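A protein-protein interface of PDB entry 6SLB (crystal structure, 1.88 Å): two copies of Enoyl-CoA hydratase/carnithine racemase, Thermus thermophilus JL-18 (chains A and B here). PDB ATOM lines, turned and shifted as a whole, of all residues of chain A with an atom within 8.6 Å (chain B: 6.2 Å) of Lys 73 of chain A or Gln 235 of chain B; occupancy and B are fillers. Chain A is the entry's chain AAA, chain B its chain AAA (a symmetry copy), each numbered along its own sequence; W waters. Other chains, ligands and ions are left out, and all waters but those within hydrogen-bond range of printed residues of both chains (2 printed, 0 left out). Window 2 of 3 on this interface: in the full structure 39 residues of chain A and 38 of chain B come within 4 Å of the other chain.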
ATOM      1  N   PHE A  69      14.945  23.145 -22.622  1.00  0.00           N
ATOM      2  CA  PHE A  69      16.032  22.906 -23.619  1.00  0.00           C
ATOM      3  C   PHE A  69      15.890  21.489 -24.199  1.00  0.00           C
ATOM      4  O   PHE A  69      16.008  20.489 -23.449  1.00  0.00           O
ATOM      5  CB  PHE A  69      17.413  23.178 -23.002  1.00  0.00           C
ATOM      6  CG  PHE A  69      18.012  22.050 -22.192  1.00  0.00           C
ATOM      7  CD1 PHE A  69      17.587  21.804 -20.890  1.00  0.00           C
ATOM      8  CD2 PHE A  69      19.002  21.236 -22.728  1.00  0.00           C
ATOM      9  CE1 PHE A  69      18.134  20.767 -20.150  1.00  0.00           C
ATOM     10  CE2 PHE A  69      19.547  20.197 -21.988  1.00  0.00           C
ATOM     11  CZ  PHE A  69      19.114  19.969 -20.701  1.00  0.00           C
ATOM     12  N   GLY A  70      15.646  21.408 -25.511  1.00  0.00           N
ATOM     13  CA  GLY A  70      15.159  20.194 -26.193  1.00  0.00           C
ATOM     14  C   GLY A  70      16.271  19.397 -26.852  1.00  0.00           C
ATOM     15  O   GLY A  70      16.425  19.511 -28.085  1.00  0.00           O
ATOM     16  N   ASP A  71      17.027  18.630 -26.058  1.00  0.00           N
ATOM     17  CA  ASP A  71      17.922  17.528 -26.514  1.00  0.00           C
ATOM     18  C   ASP A  71      19.070  18.047 -27.392  1.00  0.00           C
ATOM     19  O   ASP A  71      19.896  17.216 -27.808  1.00  0.00           O
ATOM     20  CB  ASP A  71      17.134  16.461 -27.282  1.00  0.00           C
ATOM     21  CG  ASP A  71      15.971  15.877 -26.497  1.00  0.00           C
ATOM     22  OD1 ASP A  71      15.000  16.620 -26.243  1.00  0.00           O
ATOM     23  OD2 ASP A  71      16.053  14.687 -26.133  1.00  0.00           O
ATOM     24  N   ARG A  72      19.129  19.355 -27.660  1.00  0.00           N
ATOM     25  CA  ARG A  72      20.166  19.983 -28.522  1.00  0.00           C
ATOM     26  C   ARG A  72      21.460  20.145 -27.710  1.00  0.00           C
ATOM     27  O   ARG A  72      21.377  20.147 -26.463  1.00  0.00           O
ATOM     28  CB  ARG A  72      19.661  21.334 -29.031  1.00  0.00           C
ATOM     29  CG  ARG A  72      20.326  21.791 -30.319  1.00  0.00           C
ATOM     30  CD  ARG A  72      20.268  23.295 -30.478  1.00  0.00           C
ATOM     31  NE  ARG A  72      19.876  23.651 -31.830  1.00  0.00           N
ATOM     32  CZ  ARG A  72      19.757  24.890 -32.290  1.00  0.00           C
ATOM     33  NH1 ARG A  72      20.010  25.928 -31.511  1.00  0.00           N
ATOM     34  NH2 ARG A  72      19.385  25.081 -33.540  1.00  0.00           N
ATOM     35  N   LYS A  73      22.610  20.267 -28.385  1.00  0.00           N
ATOM     36  CA  LYS A  73      23.911  20.611 -27.747  1.00  0.00           C
ATOM     37  C   LYS A  73      23.714  21.891 -26.935  1.00  0.00           C
ATOM     38  O   LYS A  73      23.600  22.972 -27.513  1.00  0.00           O
ATOM     39  CB  LYS A  73      25.014  20.800 -28.796  1.00  0.00           C
ATOM     40  CG  LYS A  73      26.423  20.956 -28.239  1.00  0.00           C
ATOM     41  CD  LYS A  73      27.108  19.631 -27.936  1.00  0.00           C
ATOM     42  CE  LYS A  73      28.623  19.712 -27.917  1.00  0.00           C
ATOM     43  NZ  LYS A  73      29.251  18.602 -28.674  1.00  0.00           N
ATOM     44  N   PRO A  74      23.660  21.821 -25.581  1.00  0.00           N
ATOM     45  CA  PRO A  74      23.356  23.004 -24.777  1.00  0.00           C
ATOM     46  C   PRO A  74      24.543  23.979 -24.792  1.00  0.00           C
ATOM     47  O   PRO A  74      25.690  23.535 -24.770  1.00  0.00           O
ATOM     48  CB  PRO A  74      23.098  22.432 -23.376  1.00  0.00           C
ATOM     49  CG  PRO A  74      23.974  21.197 -23.332  1.00  0.00           C
ATOM     50  CD  PRO A  74      23.957  20.646 -24.747  1.00  0.00           C
ATOM     51  N   ASP A  75      24.236  25.273 -24.873  1.00  0.00           N
ATOM     52  CA  ASP A  75      25.221  26.378 -24.791  1.00  0.00           C
ATOM     53  C   ASP A  75      24.888  27.199 -23.549  1.00  0.00           C
ATOM     54  O   ASP A  75      24.239  28.281 -23.684  1.00  0.00           O
ATOM     55  CB  ASP A  75      25.228  27.246 -26.047  1.00  0.00           C
ATOM     56  CG  ASP A  75      26.433  28.163 -26.089  1.00  0.00           C
ATOM     57  OD1 ASP A  75      27.090  28.326 -25.035  1.00  0.00           O
ATOM     58  OD2 ASP A  75      26.720  28.698 -27.166  1.00  0.00           O
ATOM     59  N   TYR A  76      25.318  26.699 -22.390  1.00  0.00           N
ATOM     60  CA  TYR A  76      25.044  27.332 -21.073  1.00  0.00           C
ATOM     61  C   TYR A  76      25.845  28.628 -20.933  1.00  0.00           C
ATOM     62  O   TYR A  76      25.345  29.553 -20.244  1.00  0.00           O
ATOM     63  CB  TYR A  76      25.278  26.327 -19.948  1.00  0.00           C
ATOM     64  CG  TYR A  76      24.254  25.220 -19.943  1.00  0.00           C
ATOM     65  CD1 TYR A  76      22.987  25.425 -20.472  1.00  0.00           C
ATOM     66  CD2 TYR A  76      24.535  23.973 -19.413  1.00  0.00           C
ATOM     67  CE1 TYR A  76      22.031  24.427 -20.471  1.00  0.00           C
ATOM     68  CE2 TYR A  76      23.590  22.961 -19.408  1.00  0.00           C
ATOM     69  CZ  TYR A  76      22.332  23.188 -19.943  1.00  0.00           C
ATOM     70  OH  TYR A  76      21.371  22.218 -19.965  1.00  0.00           O
ATOM     71  N   GLU A  77      27.029  28.713 -21.545  1.00  0.00           N
ATOM     72  CA  GLU A  77      27.830  29.968 -21.472  1.00  0.00           C
ATOM     73  C   GLU A  77      26.984  31.122 -22.042  1.00  0.00           C
ATOM     74  O   GLU A  77      26.909  32.223 -21.390  1.00  0.00           O
ATOM     75  CB  GLU A  77      29.189  29.832 -22.153  1.00  0.00           C
ATOM     76  CG  GLU A  77      30.187  30.812 -21.566  1.00  0.00           C
ATOM     77  CD  GLU A  77      31.465  31.120 -22.321  1.00  0.00           C
ATOM     78  OE1 GLU A  77      32.202  30.178 -22.673  1.00  0.00           O
ATOM     79  OE2 GLU A  77      31.740  32.325 -22.488  1.00  0.00           O
ATOM     80  N   GLY A 135      24.731  17.047 -13.016  1.00  0.00           N
ATOM     81  CA  GLY A 135      26.108  17.112 -13.562  1.00  0.00           C
ATOM     82  C   GLY A 135      26.528  18.520 -13.914  1.00  0.00           C
ATOM     83  O   GLY A 135      27.386  18.653 -14.773  1.00  0.00           O
ATOM     84  N   LEU A 136      25.979  19.538 -13.237  1.00  0.00           N
ATOM     85  CA  LEU A 136      26.262  20.968 -13.485  1.00  0.00           C
ATOM     86  C   LEU A 136      26.910  21.588 -12.246  1.00  0.00           C
ATOM     87  O   LEU A 136      26.903  20.962 -11.164  1.00  0.00           O
ATOM     88  CB  LEU A 136      24.967  21.705 -13.803  1.00  0.00           C
ATOM     89  CG  LEU A 136      24.335  21.333 -15.133  1.00  0.00           C
ATOM     90  CD1 LEU A 136      23.113  22.179 -15.362  1.00  0.00           C
ATOM     91  CD2 LEU A 136      25.339  21.483 -16.274  1.00  0.00           C
ATOM     92  N   GLN B 230      30.021  26.390 -16.566  1.00  0.00           N
ATOM     93  CA  GLN B 230      28.704  25.742 -16.809  1.00  0.00           C
ATOM     94  C   GLN B 230      28.594  25.351 -18.285  1.00  0.00           C
ATOM     95  O   GLN B 230      28.095  24.272 -18.562  1.00  0.00           O
ATOM     96  CB  GLN B 230      27.540  26.648 -16.426  1.00  0.00           C
ATOM     97  CG  GLN B 230      26.224  25.885 -16.342  1.00  0.00           C
ATOM     98  CD  GLN B 230      26.173  25.061 -15.075  1.00  0.00           C
ATOM     99  OE1 GLN B 230      26.905  24.076 -14.934  1.00  0.00           O
ATOM    100  NE2 GLN B 230      25.305  25.461 -14.147  1.00  0.00           N
ATOM    101  N   GLY B 231      29.121  26.184 -19.179  1.00  0.00           N
ATOM    102  CA  GLY B 231      29.361  25.824 -20.589  1.00  0.00           C
ATOM    103  C   GLY B 231      30.081  24.500 -20.737  1.00  0.00           C
ATOM    104  O   GLY B 231      29.614  23.634 -21.484  1.00  0.00           O
ATOM    105  N   GLN B 232      31.194  24.330 -20.041  1.00  0.00           N
ATOM    106  CA  GLN B 232      31.998  23.078 -20.075  1.00  0.00           C
ATOM    107  C   GLN B 232      31.224  21.913 -19.444  1.00  0.00           C
ATOM    108  O   GLN B 232      31.148  20.846 -20.070  1.00  0.00           O
ATOM    109  CB  GLN B 232      33.333  23.277 -19.368  1.00  0.00           C
ATOM    110  CG  GLN B 232      34.225  24.304 -20.072  1.00  0.00           C
ATOM    111  CD  GLN B 232      35.507  24.546 -19.318  1.00  0.00           C
ATOM    112  OE1 GLN B 232      35.912  23.731 -18.496  1.00  0.00           O
ATOM    113  NE2 GLN B 232      36.146  25.677 -19.604  1.00  0.00           N
ATOM    114  N   ALA B 233      30.622  22.084 -18.262  1.00  0.00           N
ATOM    115  CA  ALA B 233      29.815  21.011 -17.633  1.00  0.00           C
ATOM    116  C   ALA B 233      28.632  20.639 -18.548  1.00  0.00           C
ATOM    117  O   ALA B 233      28.282  19.465 -18.602  1.00  0.00           O
ATOM    118  CB  ALA B 233      29.308  21.428 -16.263  1.00  0.00           C
ATOM    119  N   GLY B 234      27.995  21.632 -19.161  1.00  0.00           N
ATOM    120  CA  GLY B 234      26.867  21.462 -20.096  1.00  0.00           C
ATOM    121  C   GLY B 234      27.204  20.558 -21.274  1.00  0.00           C
ATOM    122  O   GLY B 234      26.286  19.867 -21.755  1.00  0.00           O
ATOM    123  N   GLN B 235      28.468  20.538 -21.713  1.00  0.00           N
ATOM    124  CA  GLN B 235      28.943  19.721 -22.867  1.00  0.00           C
ATOM    125  C   GLN B 235      29.295  18.285 -22.452  1.00  0.00           C
ATOM    126  O   GLN B 235      29.589  17.494 -23.346  1.00  0.00           O
ATOM    127  CB  GLN B 235      30.186  20.357 -23.509  1.00  0.00           C
ATOM    128  CG  GLN B 235      29.952  21.776 -24.002  1.00  0.00           C
ATOM    129  CD  GLN B 235      29.399  21.813 -25.400  1.00  0.00           C
ATOM    130  OE1 GLN B 235      28.187  21.854 -25.613  1.00  0.00           O
ATOM    131  NE2 GLN B 235      30.299  21.779 -26.366  1.00  0.00           N
ATOM    132  N   THR B 236      29.274  17.926 -21.172  1.00  0.00           N
ATOM    133  CA  THR B 236      29.709  16.585 -20.706  1.00  0.00           C
ATOM    134  C   THR B 236      28.592  15.576 -20.964  1.00  0.00           C
ATOM    135  O   THR B 236      27.380  15.973 -20.957  1.00  0.00           O
ATOM    136  CB  THR B 236      30.118  16.591 -19.231  1.00  0.00           C
ATOM    137  OG1 THR B 236      28.924  16.824 -18.469  1.00  0.00           O
ATOM    138  CG2 THR B 236      31.207  17.605 -18.945  1.00  0.00           C
ATOM    139  N   GLN B 237      28.969  14.312 -21.146  1.00  0.00           N
ATOM    140  CA  GLN B 237      28.028  13.180 -21.291  1.00  0.00           C
ATOM    141  C   GLN B 237      27.215  13.065 -19.994  1.00  0.00           C
ATOM    142  O   GLN B 237      26.040  12.778 -20.053  1.00  0.00           O
ATOM    143  CB  GLN B 237      28.800  11.907 -21.641  1.00  0.00           C
ATOM    144  CG  GLN B 237      29.240  11.909 -23.101  1.00  0.00           C
ATOM    145  CD  GLN B 237      29.988  10.668 -23.533  1.00  0.00           C
ATOM    146  OE1 GLN B 237      29.999   9.635 -22.860  1.00  0.00           O
ATOM    147  NE2 GLN B 237      30.627  10.769 -24.691  1.00  0.00           N
ATOM    148  N   HIS B 239      26.206  15.500 -17.916  1.00  0.00           N
ATOM    149  CA  HIS B 239      25.088  16.467 -17.921  1.00  0.00           C
ATOM    150  C   HIS B 239      23.893  15.865 -18.667  1.00  0.00           C
ATOM    151  O   HIS B 239      22.780  15.892 -18.113  1.00  0.00           O
ATOM    152  CB  HIS B 239      25.473  17.812 -18.520  1.00  0.00           C
ATOM    153  CG  HIS B 239      24.263  18.673 -18.561  1.00  0.00           C
ATOM    154  ND1 HIS B 239      23.434  18.784 -17.462  1.00  0.00           N
ATOM    155  CD2 HIS B 239      23.665  19.358 -19.561  1.00  0.00           C
ATOM    156  CE1 HIS B 239      22.419  19.582 -17.783  1.00  0.00           C
ATOM    157  NE2 HIS B 239      22.537  19.938 -19.036  1.00  0.00           N
ATOM    158  N   GLU B 240      24.137  15.273 -19.840  1.00  0.00           N
ATOM    159  CA  GLU B 240      23.054  14.694 -20.681  1.00  0.00           C
ATOM    160  C   GLU B 240      22.404  13.546 -19.895  1.00  0.00           C
ATOM    161  O   GLU B 240      21.158  13.487 -19.872  1.00  0.00           O
ATOM    162  CB  GLU B 240      23.586  14.250 -22.050  1.00  0.00           C
ATOM    163  CG  GLU B 240      24.397  15.325 -22.761  1.00  0.00           C
ATOM    164  CD  GLU B 240      25.027  14.947 -24.101  1.00  0.00           C
ATOM    165  OE1 GLU B 240      24.852  13.795 -24.552  1.00  0.00           O
ATOM    166  OE2 GLU B 240      25.712  15.823 -24.699  1.00  0.00           O
ATOM    167  N   ARG B 257      32.627  12.207 -17.448  1.00  0.00           N
ATOM    168  CA  ARG B 257      32.956  12.828 -18.765  1.00  0.00           C
ATOM    169  C   ARG B 257      31.667  13.359 -19.426  1.00  0.00           C
ATOM    170  O   ARG B 257      30.668  13.044 -18.627  1.00  0.00           O
ATOM    171  CB  ARG B 257      33.669  11.791 -19.655  1.00  0.00           C
ATOM    172  CG  ARG B 257      32.752  10.696 -20.180  1.00  0.00           C
ATOM    173  CD  ARG B 257      33.425   9.654 -21.075  1.00  0.00           C
ATOM    174  NE  ARG B 257      33.191   9.925 -22.499  1.00  0.00           N
ATOM    175  CZ  ARG B 257      34.006  10.620 -23.291  1.00  0.00           C
ATOM    176  NH1 ARG B 257      35.140  11.117 -22.823  1.00  0.00           N
ATOM    177  NH2 ARG B 257      33.691  10.809 -24.560  1.00  0.00           N
HETATM  178  O   HOH W   1      26.856  24.163 -22.456  1.00  0.00           O
HETATM  179  O   HOH W   2      29.287  16.789 -15.533  1.00  0.00           O
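The backbone carbonyl oxygen of Pro 74 of chain A lies close to the side-chain amide oxygen of Gln 235 of chain B (3.1 Å). The side-chain hydroxyl (OH) of Tyr 76 of chain A is in hydrogen-bond range of a ring nitrogen (NE2) of His 239 of chain B (2.7 Å).
The backbone carbonyl oxygen (O) of Ala 233 of chain B sits at hydrogen-bond distance from the side-chain hydroxyl (OG1) of Thr 236 of chain B, at 2.7 Å. OG1 of Thr 236 of chain B sits at hydrogen-bond distance from N of His 239 of chain B (3.1 Å).
Among the printed residues, merely in contact across the chains: Lys 73 of chain A with Gln 235 of chain B (3.1 Å), Pro 74 of chain A with Gly 234 of chain B (3.1 Å), Leu 136 of chain A with Gln 230 of chain B (3.3 Å), Tyr 76 of chain A with Gly 234 of chain B (3.5 Å), Leu 136 of chain A with His 239 of chain B (3.5 Å), Tyr 76 of chain A with Gln 230 of chain B (3.7 Å), Gly 135 of chain A with Ala 233 of chain B (3.7 Å), Phe 69 of chain A with His 239 of chain B (3.8 Å), Glu 77 of chain A with Gly 231 of chain B (3.8 Å), Tyr 76 of chain A with Gly 231 of chain B (3.9 Å), Leu 136 of chain A with Gly 234 of chain B (3.9 Å) and Leu 136 of chain A with Ala 233 of chain B (3.97 Å).
Printed residues of chain B within 4 Å of Lys 73 of chain A: Gln 235 (3.1 Å). Asp 75 of chain A touches none of the printed residues of chain B. Of the printed residues of chain B, Glu 77 of chain A touches Gly 231 (3.8 Å). Printed residues of chain B within 4 Å of Gly 135 of chain A: Ala 233 (3.7 Å). Of the printed residues of chain B, Leu 136 of chain A touches Gln 230 (3.3 Å), Ala 233 (3.97 Å), Gly 234 (3.9 Å) and His 239 (3.5 Å). Of the printed residues of chain A, Gln 230 of chain B touches Tyr 76 (3.7 Å) and Leu 136 (3.3 Å). Of the printed residues of chain A, Ala 233 of chain B touches Gly 135 and Leu 136. Gly 234 of chain B touches three residues of chain A. No residue of chain A comes within 4 Å of Thr 236 of chain B. Arg 257 of chain B touches none of the printed residues of chain A. The nearest residue of chain B that does not touch Lys 73 of chain A is Glu 240 of chain B (5.2 Å). The nearest residue of chain A that does not touch Gln 235 of chain B is Asp 75 of chain A (5.3 Å).
Printed residues of chain B that touch a printed residue of chain A: Gln 230, Gly 231, Ala 233, Gly 234, Gln 235 and His 239. Hydrophobic or aromatic side chains of chain B that line the printed part of chain A: Ala 233 and His 239. Of the 11 printed residues of chain A, 7 touch a printed residue of chain B. Printed residues of chain A that touch a printed residue of chain B: Phe 69, Lys 73, Pro 74, Tyr 76, Glu 77, Gly 135 and Leu 136. Hydrophobic or aromatic side chains of chain A within 4 Å of the printed part of chain B: Phe 69, Pro 74, Tyr 76 and Leu 136.
No position is printed for both chains.
Water W1 lies within hydrogen-bond range of the backbone carbonyl oxygen (O) of Pro 74 of chain A, the backbone NH (N) of Tyr 76 of chain A and the backbone carbonyl oxygen (O) of Gly 231 of chain B. Water W2 lies within hydrogen-bond range of O of Gly 135 of chain A (2.8 Å) and OG1 of Thr 236 of chain B (3.0 Å).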
